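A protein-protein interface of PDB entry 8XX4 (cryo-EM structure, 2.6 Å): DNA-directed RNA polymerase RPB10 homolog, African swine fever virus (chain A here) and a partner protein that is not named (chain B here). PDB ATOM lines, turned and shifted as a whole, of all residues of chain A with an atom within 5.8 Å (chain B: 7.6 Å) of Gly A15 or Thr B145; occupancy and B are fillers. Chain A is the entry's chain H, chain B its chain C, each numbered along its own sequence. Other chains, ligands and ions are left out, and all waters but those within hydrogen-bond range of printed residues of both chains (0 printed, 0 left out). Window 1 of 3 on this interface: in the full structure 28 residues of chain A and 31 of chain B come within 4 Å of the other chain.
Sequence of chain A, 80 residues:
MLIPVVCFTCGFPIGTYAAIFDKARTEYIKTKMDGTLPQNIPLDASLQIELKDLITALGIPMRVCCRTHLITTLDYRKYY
OG1 of Thr B145 sits at hydrogen-bond distance from O of Thr A16, 2.7 Å away.
The guanidinium group (NH1) of Arg B95 sits at hydrogen-bond distance from the backbone carbonyl oxygen (O) of Ile A3 (2.9 Å).
O of Leu B37 sits at hydrogen-bond distance from ND2 of Asn B143 (2.7 Å).
The backbone carbonyl oxygen (O) of Leu B28 sits at hydrogen-bond distance from the guanidinium group (NH2) of Arg B127 (3.2 Å).
O of Val A5 is in hydrogen-bond range of N of Ile A14 (3.5 Å).
N of Gly A15 sits at hydrogen-bond distance from O of Val A5, at 2.7 Å.
The backbone NH of Ser B126 sits at hydrogen-bond distance from the backbone carbonyl oxygen of Phe B146 (2.9 Å).
The backbone carbonyl oxygen (O) of Pro A13 lies within hydrogen-bond range of the side-chain hydroxyl (OG1) of Thr A16, at 2.9 Å.
Among the printed residues, pairs that only touch across the chains: Val A5 with Phe B98 (3.1 Å), Thr A16 with Phe B146 (3.2 Å), Val A6 with Phe B98 (3.3 Å), Thr A16 with Asn B143 (3.3 Å), Val A5 with Arg B95 (3.3 Å), Ala A19 with Glu B147 (3.5 Å), Ile A20 with Phe B29 (3.5 Å), Gly A15 with Phe B146 (3.5 Å), Pro A4 with Arg B95 (3.6 Å), Val A5 with Phe B146 (3.6 Å), Pro A13 with Pro B100 (3.6 Å), Thr A16 with Leu B35 (3.6 Å), Gly A15 with Thr B145 (3.7 Å), Ala A18 with Glu B147 (3.8 Å), Ala A19 with Leu B28 (3.9 Å) and Ala A19 with Phe B29 (3.99 Å).
Of the 14 printed residues of chain A, 10 touch a printed residue of chain B.
Hydrophobic or aromatic side chains of chain A within 4 Å of the printed part of chain B: Val A5, Val A6, Pro A13, Ala A18, Ala A19 and Ile A20.
Of the 23 printed residues of chain B, 10 touch a printed residue of chain A.
Printed residues of chain B that touch a printed residue of chain A: Leu B28, Phe B29, Leu B35, Arg B95, Phe B98, Pro B100, Asn B143, Thr B145, Phe B146 and Glu B147.
Hydrophobic or aromatic side chains of chain B within 4 Å of the printed part of chain A: Leu B28, Phe B29, Leu B35, Phe B98, Pro B100 and Phe B146.
Among the printed residues, no Asp or Glu carboxylate lies within 4 Å of a Lys or Arg side-chain nitrogen of the other chain.
Of the printed residues of chain B, Thr A16 touches Leu B35 (3.6 Å), Asn B143 (3.3 Å), Thr B145 (2.7 Å) and Phe B146 (3.2 Å).
Printed residues of chain A within 4 Å of Pro B100: Pro A13 (3.6 Å).
Thr B123 touches none of the printed residues of chain A.
Thr B145 touches two residues of chain A.
Printed residues of chain A within 4 Å of Phe B146: Val A5 (3.6 Å), Gly A15 (3.5 Å) and Thr A16 (3.2 Å).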
ATOM      1  N   ILE A   3     -17.167 -32.593   7.453  1.00  0.00           N
ATOM      2  CA  ILE A   3     -17.319 -33.036   6.065  1.00  0.00           C
ATOM      3  C   ILE A   3     -16.205 -32.411   5.240  1.00  0.00           C
ATOM      4  O   ILE A   3     -15.958 -31.196   5.360  1.00  0.00           O
ATOM      5  CB  ILE A   3     -18.703 -32.646   5.516  1.00  0.00           C
ATOM      6  CG1 ILE A   3     -19.785 -33.528   6.126  1.00  0.00           C
ATOM      7  CG2 ILE A   3     -18.746 -32.772   4.008  1.00  0.00           C
ATOM      8  CD1 ILE A   3     -21.142 -32.894   6.142  1.00  0.00           C
ATOM      9  N   PRO A   4     -15.489 -33.174   4.417  1.00  0.00           N
ATOM     10  CA  PRO A   4     -14.325 -32.612   3.728  1.00  0.00           C
ATOM     11  C   PRO A   4     -14.724 -31.481   2.796  1.00  0.00           C
ATOM     12  O   PRO A   4     -15.870 -31.378   2.359  1.00  0.00           O
ATOM     13  CB  PRO A   4     -13.761 -33.806   2.953  1.00  0.00           C
ATOM     14  CG  PRO A   4     -14.899 -34.746   2.834  1.00  0.00           C
ATOM     15  CD  PRO A   4     -15.690 -34.591   4.082  1.00  0.00           C
ATOM     16  N   VAL A   5     -13.761 -30.603   2.523  1.00  0.00           N
ATOM     17  CA  VAL A   5     -14.022 -29.471   1.642  1.00  0.00           C
ATOM     18  C   VAL A   5     -14.383 -29.959   0.247  1.00  0.00           C
ATOM     19  O   VAL A   5     -15.343 -29.479  -0.367  1.00  0.00           O
ATOM     20  CB  VAL A   5     -12.811 -28.525   1.622  1.00  0.00           C
ATOM     21  CG1 VAL A   5     -12.978 -27.497   0.542  1.00  0.00           C
ATOM     22  CG2 VAL A   5     -12.663 -27.848   2.959  1.00  0.00           C
ATOM     23  N   VAL A   6     -13.633 -30.924  -0.270  1.00  0.00           N
ATOM     24  CA  VAL A   6     -13.932 -31.543  -1.549  1.00  0.00           C
ATOM     25  C   VAL A   6     -14.066 -33.040  -1.323  1.00  0.00           C
ATOM     26  O   VAL A   6     -13.529 -33.597  -0.366  1.00  0.00           O
ATOM     27  CB  VAL A   6     -12.857 -31.250  -2.613  1.00  0.00           C
ATOM     28  CG1 VAL A   6     -12.890 -29.793  -3.013  1.00  0.00           C
ATOM     29  CG2 VAL A   6     -11.497 -31.627  -2.095  1.00  0.00           C
ATOM     30  N   CYS A   7     -14.808 -33.686  -2.217  1.00  0.00           N
ATOM     31  CA  CYS A   7     -14.957 -35.132  -2.156  1.00  0.00           C
ATOM     32  C   CYS A   7     -13.595 -35.800  -2.253  1.00  0.00           C
ATOM     33  O   CYS A   7     -12.802 -35.487  -3.143  1.00  0.00           O
ATOM     34  CB  CYS A   7     -15.869 -35.604  -3.285  1.00  0.00           C
ATOM     35  SG  CYS A   7     -15.759 -37.346  -3.691  1.00  0.00           S
ATOM     36  N   PHE A  12     -14.864 -33.104  -6.148  1.00  0.00           N
ATOM     37  CA  PHE A  12     -16.009 -32.218  -6.240  1.00  0.00           C
ATOM     38  C   PHE A  12     -16.223 -31.510  -4.905  1.00  0.00           C
ATOM     39  O   PHE A  12     -16.179 -32.144  -3.848  1.00  0.00           O
ATOM     40  CB  PHE A  12     -17.263 -32.997  -6.623  1.00  0.00           C
ATOM     41  CG  PHE A  12     -18.455 -32.129  -6.881  1.00  0.00           C
ATOM     42  CD1 PHE A  12     -18.687 -31.608  -8.137  1.00  0.00           C
ATOM     43  CD2 PHE A  12     -19.345 -31.830  -5.864  1.00  0.00           C
ATOM     44  CE1 PHE A  12     -19.778 -30.811  -8.373  1.00  0.00           C
ATOM     45  CE2 PHE A  12     -20.434 -31.030  -6.097  1.00  0.00           C
ATOM     46  CZ  PHE A  12     -20.652 -30.520  -7.350  1.00  0.00           C
ATOM     47  N   PRO A  13     -16.465 -30.205  -4.916  1.00  0.00           N
ATOM     48  CA  PRO A  13     -16.606 -29.441  -3.662  1.00  0.00           C
ATOM     49  C   PRO A  13     -17.940 -29.641  -2.944  1.00  0.00           C
ATOM     50  O   PRO A  13     -18.873 -28.853  -3.037  1.00  0.00           O
ATOM     51  CB  PRO A  13     -16.435 -27.998  -4.135  1.00  0.00           C
ATOM     52  CG  PRO A  13     -16.925 -28.014  -5.526  1.00  0.00           C
ATOM     53  CD  PRO A  13     -16.526 -29.332  -6.098  1.00  0.00           C
ATOM     54  N   ILE A  14     -18.033 -30.736  -2.189  1.00  0.00           N
ATOM     55  CA  ILE A  14     -19.192 -30.951  -1.330  1.00  0.00           C
ATOM     56  C   ILE A  14     -19.134 -30.093  -0.074  1.00  0.00           C
ATOM     57  O   ILE A  14     -20.162 -29.898   0.591  1.00  0.00           O
ATOM     58  CB  ILE A  14     -19.314 -32.435  -0.949  1.00  0.00           C
ATOM     59  CG1 ILE A  14     -17.969 -32.971  -0.465  1.00  0.00           C
ATOM     60  CG2 ILE A  14     -19.814 -33.244  -2.126  1.00  0.00           C
ATOM     61  CD1 ILE A  14     -18.068 -34.214   0.362  1.00  0.00           C
ATOM     62  N   GLY A  15     -17.958 -29.567   0.270  1.00  0.00           N
ATOM     63  CA  GLY A  15     -17.848 -28.686   1.415  1.00  0.00           C
ATOM     64  C   GLY A  15     -18.555 -27.366   1.232  1.00  0.00           C
ATOM     65  O   GLY A  15     -18.802 -26.667   2.217  1.00  0.00           O
ATOM     66  N   THR A  16     -18.879 -27.007  -0.010  1.00  0.00           N
ATOM     67  CA  THR A  16     -19.678 -25.814  -0.249  1.00  0.00           C
ATOM     68  C   THR A  16     -21.040 -25.940   0.410  1.00  0.00           C
ATOM     69  O   THR A  16     -21.568 -24.971   0.965  1.00  0.00           O
ATOM     70  CB  THR A  16     -19.844 -25.582  -1.749  1.00  0.00           C
ATOM     71  OG1 THR A  16     -18.658 -25.993  -2.434  1.00  0.00           O
ATOM     72  CG2 THR A  16     -20.087 -24.125  -2.025  1.00  0.00           C
ATOM     73  N   TYR A  17     -21.622 -27.131   0.358  1.00  0.00           N
ATOM     74  CA  TYR A  17     -22.940 -27.385   0.910  1.00  0.00           C
ATOM     75  C   TYR A  17     -22.893 -28.267   2.145  1.00  0.00           C
ATOM     76  O   TYR A  17     -23.936 -28.758   2.570  1.00  0.00           O
ATOM     77  CB  TYR A  17     -23.830 -28.028  -0.150  1.00  0.00           C
ATOM     78  CG  TYR A  17     -23.500 -27.602  -1.556  1.00  0.00           C
ATOM     79  CD1 TYR A  17     -23.927 -26.380  -2.050  1.00  0.00           C
ATOM     80  CD2 TYR A  17     -22.756 -28.420  -2.391  1.00  0.00           C
ATOM     81  CE1 TYR A  17     -23.627 -25.989  -3.333  1.00  0.00           C
ATOM     82  CE2 TYR A  17     -22.449 -28.038  -3.674  1.00  0.00           C
ATOM     83  CZ  TYR A  17     -22.887 -26.822  -4.143  1.00  0.00           C
ATOM     84  OH  TYR A  17     -22.584 -26.437  -5.426  1.00  0.00           O
ATOM     85  N   ALA A  18     -21.709 -28.496   2.717  1.00  0.00           N
ATOM     86  CA  ALA A  18     -21.601 -29.344   3.903  1.00  0.00           C
ATOM     87  C   ALA A  18     -22.468 -28.837   5.052  1.00  0.00           C
ATOM     88  O   ALA A  18     -23.226 -29.606   5.655  1.00  0.00           O
ATOM     89  CB  ALA A  18     -20.141 -29.435   4.339  1.00  0.00           C
ATOM     90  N   ALA A  19     -22.370 -27.546   5.376  1.00  0.00           N
ATOM     91  CA  ALA A  19     -23.104 -27.010   6.523  1.00  0.00           C
ATOM     92  C   ALA A  19     -24.605 -26.992   6.268  1.00  0.00           C
ATOM     93  O   ALA A  19     -25.402 -27.387   7.137  1.00  0.00           O
ATOM     94  CB  ALA A  19     -22.606 -25.606   6.848  1.00  0.00           C
ATOM     95  N   ILE A  20     -25.007 -26.516   5.089  1.00  0.00           N
ATOM     96  CA  ILE A  20     -26.416 -26.512   4.723  1.00  0.00           C
ATOM     97  C   ILE A  20     -26.967 -27.924   4.768  1.00  0.00           C
ATOM     98  O   ILE A  20     -28.075 -28.155   5.259  1.00  0.00           O
ATOM     99  CB  ILE A  20     -26.610 -25.871   3.337  1.00  0.00           C
ATOM    100  CG1 ILE A  20     -26.136 -24.420   3.347  1.00  0.00           C
ATOM    101  CG2 ILE A  20     -28.059 -25.949   2.911  1.00  0.00           C
ATOM    102  CD1 ILE A  20     -25.832 -23.868   1.976  1.00  0.00           C
ATOM    103  N   ILE B  14     -28.314 -24.726  -6.340  1.00  0.00           N
ATOM    104  CA  ILE B  14     -29.095 -25.064  -5.159  1.00  0.00           C
ATOM    105  C   ILE B  14     -30.569 -24.851  -5.459  1.00  0.00           C
ATOM    106  O   ILE B  14     -30.979 -23.773  -5.906  1.00  0.00           O
ATOM    107  CB  ILE B  14     -28.648 -24.216  -3.960  1.00  0.00           C
ATOM    108  CG1 ILE B  14     -27.125 -24.095  -3.929  1.00  0.00           C
ATOM    109  CG2 ILE B  14     -29.157 -24.811  -2.676  1.00  0.00           C
ATOM    110  CD1 ILE B  14     -26.611 -23.168  -2.857  1.00  0.00           C
ATOM    111  N   ALA B  25     -30.091 -22.650   4.632  1.00  0.00           N
ATOM    112  CA  ALA B  25     -29.279 -21.605   4.022  1.00  0.00           C
ATOM    113  C   ALA B  25     -29.636 -20.241   4.593  1.00  0.00           C
ATOM    114  O   ALA B  25     -28.753 -19.445   4.926  1.00  0.00           O
ATOM    115  CB  ALA B  25     -29.451 -21.622   2.505  1.00  0.00           C
ATOM    116  N   LEU B  28     -28.394 -19.983   8.533  1.00  0.00           N
ATOM    117  CA  LEU B  28     -26.987 -19.964   8.909  1.00  0.00           C
ATOM    118  C   LEU B  28     -26.074 -19.279   7.903  1.00  0.00           C
ATOM    119  O   LEU B  28     -24.887 -19.118   8.191  1.00  0.00           O
ATOM    120  CB  LEU B  28     -26.485 -21.390   9.168  1.00  0.00           C
ATOM    121  CG  LEU B  28     -26.404 -22.363   8.004  1.00  0.00           C
ATOM    122  CD1 LEU B  28     -24.966 -22.543   7.621  1.00  0.00           C
ATOM    123  CD2 LEU B  28     -27.043 -23.668   8.342  1.00  0.00           C
ATOM    124  N   PHE B  29     -26.589 -18.856   6.750  1.00  0.00           N
ATOM    125  CA  PHE B  29     -25.811 -18.073   5.807  1.00  0.00           C
ATOM    126  C   PHE B  29     -26.520 -16.810   5.348  1.00  0.00           C
ATOM    127  O   PHE B  29     -25.885 -15.969   4.702  1.00  0.00           O
ATOM    128  CB  PHE B  29     -25.451 -18.910   4.569  1.00  0.00           C
ATOM    129  CG  PHE B  29     -24.425 -19.972   4.829  1.00  0.00           C
ATOM    130  CD1 PHE B  29     -23.266 -19.677   5.523  1.00  0.00           C
ATOM    131  CD2 PHE B  29     -24.608 -21.257   4.359  1.00  0.00           C
ATOM    132  CE1 PHE B  29     -22.325 -20.649   5.765  1.00  0.00           C
ATOM    133  CE2 PHE B  29     -23.662 -22.231   4.588  1.00  0.00           C
ATOM    134  CZ  PHE B  29     -22.522 -21.927   5.294  1.00  0.00           C
ATOM    135  N   LEU B  31     -28.648 -16.734   3.016  1.00  0.00           N
ATOM    136  CA  LEU B  31     -28.490 -16.918   1.581  1.00  0.00           C
ATOM    137  C   LEU B  31     -29.832 -17.312   0.984  1.00  0.00           C
ATOM    138  O   LEU B  31     -30.408 -18.336   1.363  1.00  0.00           O
ATOM    139  CB  LEU B  31     -27.430 -17.980   1.292  1.00  0.00           C
ATOM    140  CG  LEU B  31     -27.183 -18.375  -0.163  1.00  0.00           C
ATOM    141  CD1 LEU B  31     -26.126 -17.482  -0.775  1.00  0.00           C
ATOM    142  CD2 LEU B  31     -26.754 -19.822  -0.241  1.00  0.00           C
ATOM    143  N   LEU B  35     -25.126 -19.298  -5.039  1.00  0.00           N
ATOM    144  CA  LEU B  35     -23.834 -18.848  -4.555  1.00  0.00           C
ATOM    145  C   LEU B  35     -23.067 -18.140  -5.670  1.00  0.00           C
ATOM    146  O   LEU B  35     -23.324 -18.373  -6.853  1.00  0.00           O
ATOM    147  CB  LEU B  35     -23.030 -20.033  -4.032  1.00  0.00           C
ATOM    148  CG  LEU B  35     -23.505 -20.599  -2.698  1.00  0.00           C
ATOM    149  CD1 LEU B  35     -22.956 -21.990  -2.492  1.00  0.00           C
ATOM    150  CD2 LEU B  35     -23.096 -19.687  -1.564  1.00  0.00           C
ATOM    151  N   PRO B  36     -22.127 -17.259  -5.319  1.00  0.00           N
ATOM    152  CA  PRO B  36     -21.392 -16.533  -6.367  1.00  0.00           C
ATOM    153  C   PRO B  36     -20.642 -17.437  -7.327  1.00  0.00           C
ATOM    154  O   PRO B  36     -20.514 -17.103  -8.510  1.00  0.00           O
ATOM    155  CB  PRO B  36     -20.439 -15.638  -5.564  1.00  0.00           C
ATOM    156  CG  PRO B  36     -20.385 -16.233  -4.210  1.00  0.00           C
ATOM    157  CD  PRO B  36     -21.726 -16.825  -3.974  1.00  0.00           C
ATOM    158  N   LEU B  37     -20.140 -18.571  -6.852  1.00  0.00           N
ATOM    159  CA  LEU B  37     -19.395 -19.513  -7.675  1.00  0.00           C
ATOM    160  C   LEU B  37     -20.109 -20.853  -7.660  1.00  0.00           C
ATOM    161  O   LEU B  37     -20.443 -21.370  -6.591  1.00  0.00           O
ATOM    162  CB  LEU B  37     -17.961 -19.664  -7.171  1.00  0.00           C
ATOM    163  CG  LEU B  37     -17.088 -18.421  -7.322  1.00  0.00           C
ATOM    164  CD1 LEU B  37     -17.125 -17.597  -6.060  1.00  0.00           C
ATOM    165  CD2 LEU B  37     -15.677 -18.818  -7.643  1.00  0.00           C
ATOM    166  N   ARG B  95      -7.892 -28.030   4.770  1.00  0.00           N
ATOM    167  CA  ARG B  95      -9.194 -27.448   4.448  1.00  0.00           C
ATOM    168  C   ARG B  95      -9.050 -26.282   3.478  1.00  0.00           C
ATOM    169  O   ARG B  95      -9.811 -26.162   2.513  1.00  0.00           O
ATOM    170  CB  ARG B  95      -9.911 -26.971   5.712  1.00  0.00           C
ATOM    171  CG  ARG B  95      -9.886 -27.909   6.883  1.00  0.00           C
ATOM    172  CD  ARG B  95     -10.976 -28.935   6.814  1.00  0.00           C
ATOM    173  NE  ARG B  95     -12.286 -28.350   6.583  1.00  0.00           N
ATOM    174  CZ  ARG B  95     -13.379 -29.061   6.356  1.00  0.00           C
ATOM    175  NH1 ARG B  95     -13.347 -30.381   6.323  1.00  0.00           N
ATOM    176  NH2 ARG B  95     -14.530 -28.432   6.152  1.00  0.00           N
ATOM    177  N   PHE B  98      -7.972 -26.875  -0.413  1.00  0.00           N
ATOM    178  CA  PHE B  98      -8.936 -27.489  -1.308  1.00  0.00           C
ATOM    179  C   PHE B  98     -10.212 -26.684  -1.458  1.00  0.00           C
ATOM    180  O   PHE B  98     -11.186 -27.195  -2.012  1.00  0.00           O
ATOM    181  CB  PHE B  98      -9.247 -28.906  -0.841  1.00  0.00           C
ATOM    182  CG  PHE B  98      -8.177 -29.881  -1.194  1.00  0.00           C
ATOM    183  CD1 PHE B  98      -8.132 -30.445  -2.449  1.00  0.00           C
ATOM    184  CD2 PHE B  98      -7.188 -30.199  -0.288  1.00  0.00           C
ATOM    185  CE1 PHE B  98      -7.143 -31.324  -2.781  1.00  0.00           C
ATOM    186  CE2 PHE B  98      -6.196 -31.076  -0.622  1.00  0.00           C
ATOM    187  CZ  PHE B  98      -6.171 -31.639  -1.870  1.00  0.00           C
ATOM    188  N   PRO B 100     -12.151 -24.483  -3.638  1.00  0.00           N
ATOM    189  CA  PRO B 100     -12.030 -24.108  -5.051  1.00  0.00           C
ATOM    190  C   PRO B 100     -12.148 -22.604  -5.217  1.00  0.00           C
ATOM    191  O   PRO B 100     -13.129 -21.994  -4.787  1.00  0.00           O
ATOM    192  CB  PRO B 100     -13.199 -24.838  -5.719  1.00  0.00           C
ATOM    193  CG  PRO B 100     -13.668 -25.822  -4.730  1.00  0.00           C
ATOM    194  CD  PRO B 100     -13.362 -25.275  -3.389  1.00  0.00           C
ATOM    195  N   THR B 123     -18.163 -22.074  14.626  1.00  0.00           N
ATOM    196  CA  THR B 123     -17.642 -22.596  13.373  1.00  0.00           C
ATOM    197  C   THR B 123     -17.095 -21.456  12.526  1.00  0.00           C
ATOM    198  O   THR B 123     -17.788 -20.463  12.290  1.00  0.00           O
ATOM    199  CB  THR B 123     -18.730 -23.345  12.607  1.00  0.00           C
ATOM    200  OG1 THR B 123     -19.171 -24.466  13.380  1.00  0.00           O
ATOM    201  CG2 THR B 123     -18.196 -23.840  11.283  1.00  0.00           C
ATOM    202  N   ILE B 124     -15.850 -21.600  12.085  1.00  0.00           N
ATOM    203  CA  ILE B 124     -15.247 -20.650  11.161  1.00  0.00           C
ATOM    204  C   ILE B 124     -15.687 -21.005   9.750  1.00  0.00           C
ATOM    205  O   ILE B 124     -15.598 -22.164   9.335  1.00  0.00           O
ATOM    206  CB  ILE B 124     -13.716 -20.671  11.276  1.00  0.00           C
ATOM    207  CG1 ILE B 124     -13.277 -20.689  12.735  1.00  0.00           C
ATOM    208  CG2 ILE B 124     -13.115 -19.484  10.571  1.00  0.00           C
ATOM    209  CD1 ILE B 124     -12.146 -21.648  12.991  1.00  0.00           C
ATOM    210  N   TYR B 125     -16.160 -20.015   9.009  1.00  0.00           N
ATOM    211  CA  TYR B 125     -16.573 -20.218   7.630  1.00  0.00           C
ATOM    212  C   TYR B 125     -15.643 -19.466   6.691  1.00  0.00           C
ATOM    213  O   TYR B 125     -14.823 -18.649   7.110  1.00  0.00           O
ATOM    214  CB  TYR B 125     -18.021 -19.769   7.421  1.00  0.00           C
ATOM    215  CG  TYR B 125     -19.026 -20.590   8.185  1.00  0.00           C
ATOM    216  CD1 TYR B 125     -19.396 -21.850   7.748  1.00  0.00           C
ATOM    217  CD2 TYR B 125     -19.607 -20.104   9.342  1.00  0.00           C
ATOM    218  CE1 TYR B 125     -20.313 -22.602   8.441  1.00  0.00           C
ATOM    219  CE2 TYR B 125     -20.525 -20.848  10.042  1.00  0.00           C
ATOM    220  CZ  TYR B 125     -20.876 -22.096   9.589  1.00  0.00           C
ATOM    221  OH  TYR B 125     -21.791 -22.839  10.290  1.00  0.00           O
ATOM    222  N   SER B 126     -15.779 -19.762   5.398  1.00  0.00           N
ATOM    223  CA  SER B 126     -15.006 -19.054   4.389  1.00  0.00           C
ATOM    224  C   SER B 126     -15.376 -17.582   4.304  1.00  0.00           C
ATOM    225  O   SER B 126     -14.592 -16.792   3.771  1.00  0.00           O
ATOM    226  CB  SER B 126     -15.192 -19.710   3.026  1.00  0.00           C
ATOM    227  OG  SER B 126     -14.385 -20.861   2.914  1.00  0.00           O
ATOM    228  N   ARG B 127     -16.549 -17.196   4.806  1.00  0.00           N
ATOM    229  CA  ARG B 127     -16.900 -15.784   4.856  1.00  0.00           C
ATOM    230  C   ARG B 127     -16.017 -15.014   5.822  1.00  0.00           C
ATOM    231  O   ARG B 127     -15.970 -13.783   5.754  1.00  0.00           O
ATOM    232  CB  ARG B 127     -18.366 -15.614   5.248  1.00  0.00           C
ATOM    233  CG  ARG B 127     -18.698 -16.130   6.627  1.00  0.00           C
ATOM    234  CD  ARG B 127     -19.926 -15.447   7.193  1.00  0.00           C
ATOM    235  NE  ARG B 127     -20.601 -16.286   8.174  1.00  0.00           N
ATOM    236  CZ  ARG B 127     -21.909 -16.489   8.212  1.00  0.00           C
ATOM    237  NH1 ARG B 127     -22.725 -15.916   7.343  1.00  0.00           N
ATOM    238  NH2 ARG B 127     -22.413 -17.290   9.147  1.00  0.00           N
ATOM    239  N   PHE B 142     -13.982 -17.330  -3.874  1.00  0.00           N
ATOM    240  CA  PHE B 142     -14.455 -18.592  -3.335  1.00  0.00           C
ATOM    241  C   PHE B 142     -15.812 -18.372  -2.687  1.00  0.00           C
ATOM    242  O   PHE B 142     -16.183 -17.250  -2.341  1.00  0.00           O
ATOM    243  CB  PHE B 142     -13.469 -19.192  -2.323  1.00  0.00           C
ATOM    244  CG  PHE B 142     -12.980 -18.215  -1.296  1.00  0.00           C
ATOM    245  CD1 PHE B 142     -13.747 -17.906  -0.191  1.00  0.00           C
ATOM    246  CD2 PHE B 142     -11.749 -17.610  -1.434  1.00  0.00           C
ATOM    247  CE1 PHE B 142     -13.299 -17.010   0.745  1.00  0.00           C
ATOM    248  CE2 PHE B 142     -11.299 -16.714  -0.500  1.00  0.00           C
ATOM    249  CZ  PHE B 142     -12.073 -16.415   0.590  1.00  0.00           C
ATOM    250  N   ASN B 143     -16.557 -19.458  -2.537  1.00  0.00           N
ATOM    251  CA  ASN B 143     -17.841 -19.378  -1.864  1.00  0.00           C
ATOM    252  C   ASN B 143     -17.632 -19.196  -0.364  1.00  0.00           C
ATOM    253  O   ASN B 143     -16.684 -19.744   0.201  1.00  0.00           O
ATOM    254  CB  ASN B 143     -18.668 -20.631  -2.131  1.00  0.00           C
ATOM    255  CG  ASN B 143     -19.301 -20.619  -3.494  1.00  0.00           C
ATOM    256  OD1 ASN B 143     -19.782 -19.589  -3.949  1.00  0.00           O
ATOM    257  ND2 ASN B 143     -19.298 -21.759  -4.162  1.00  0.00           N
ATOM    258  N   PRO B 144     -18.496 -18.438   0.306  1.00  0.00           N
ATOM    259  CA  PRO B 144     -18.333 -18.192   1.744  1.00  0.00           C
ATOM    260  C   PRO B 144     -18.953 -19.246   2.649  1.00  0.00           C
ATOM    261  O   PRO B 144     -19.126 -18.980   3.842  1.00  0.00           O
ATOM    262  CB  PRO B 144     -19.054 -16.852   1.919  1.00  0.00           C
ATOM    263  CG  PRO B 144     -20.153 -16.908   0.919  1.00  0.00           C
ATOM    264  CD  PRO B 144     -19.665 -17.732  -0.243  1.00  0.00           C
ATOM    265  N   THR B 145     -19.287 -20.421   2.125  1.00  0.00           N
ATOM    266  CA  THR B 145     -20.048 -21.416   2.859  1.00  0.00           C
ATOM    267  C   THR B 145     -19.217 -22.606   3.314  1.00  0.00           C
ATOM    268  O   THR B 145     -19.769 -23.525   3.924  1.00  0.00           O
ATOM    269  CB  THR B 145     -21.210 -21.904   2.001  1.00  0.00           C
ATOM    270  OG1 THR B 145     -20.704 -22.384   0.753  1.00  0.00           O
ATOM    271  CG2 THR B 145     -22.170 -20.770   1.737  1.00  0.00           C
ATOM    272  N   PHE B 146     -17.921 -22.625   3.028  1.00  0.00           N
ATOM    273  CA  PHE B 146     -17.079 -23.718   3.490  1.00  0.00           C
ATOM    274  C   PHE B 146     -16.868 -23.619   4.991  1.00  0.00           C
ATOM    275  O   PHE B 146     -16.789 -22.524   5.549  1.00  0.00           O
ATOM    276  CB  PHE B 146     -15.733 -23.701   2.773  1.00  0.00           C
ATOM    277  CG  PHE B 146     -15.828 -23.969   1.308  1.00  0.00           C
ATOM    278  CD1 PHE B 146     -16.015 -22.935   0.415  1.00  0.00           C
ATOM    279  CD2 PHE B 146     -15.735 -25.256   0.823  1.00  0.00           C
ATOM    280  CE1 PHE B 146     -16.108 -23.179  -0.927  1.00  0.00           C
ATOM    281  CE2 PHE B 146     -15.827 -25.503  -0.521  1.00  0.00           C
ATOM    282  CZ  PHE B 146     -16.015 -24.462  -1.396  1.00  0.00           C
ATOM    283  N   GLU B 147     -16.786 -24.768   5.649  1.00  0.00           N
ATOM    284  CA  GLU B 147     -16.458 -24.818   7.071  1.00  0.00           C
ATOM    285  C   GLU B 147     -14.954 -24.998   7.191  1.00  0.00           C
ATOM    286  O   GLU B 147     -14.434 -26.101   7.021  1.00  0.00           O
ATOM    287  CB  GLU B 147     -17.208 -25.943   7.772  1.00  0.00           C
ATOM    288  CG  GLU B 147     -18.695 -25.950   7.536  1.00  0.00           C
ATOM    289  CD  GLU B 147     -19.365 -27.146   8.169  1.00  0.00           C
ATOM    290  OE1 GLU B 147     -19.018 -28.288   7.803  1.00  0.00           O
ATOM    291  OE2 GLU B 147     -20.240 -26.946   9.034  1.00  0.00           O
ATOM    292  N   ILE B 148     -14.250 -23.904   7.469  1.00  0.00           N
ATOM    293  CA  ILE B 148     -12.811 -23.989   7.677  1.00  0.00           C
ATOM    294  C   ILE B 148     -12.505 -24.772   8.945  1.00  0.00           C
ATOM    295  O   ILE B 148     -11.561 -25.568   8.991  1.00  0.00           O
ATOM    296  CB  ILE B 148     -12.203 -22.578   7.709  1.00  0.00           C
ATOM    297  CG1 ILE B 148     -12.418 -21.892   6.362  1.00  0.00           C
ATOM    298  CG2 ILE B 148     -10.731 -22.636   8.057  1.00  0.00           C
ATOM    299  CD1 ILE B 148     -11.727 -20.568   6.238  1.00  0.00           C
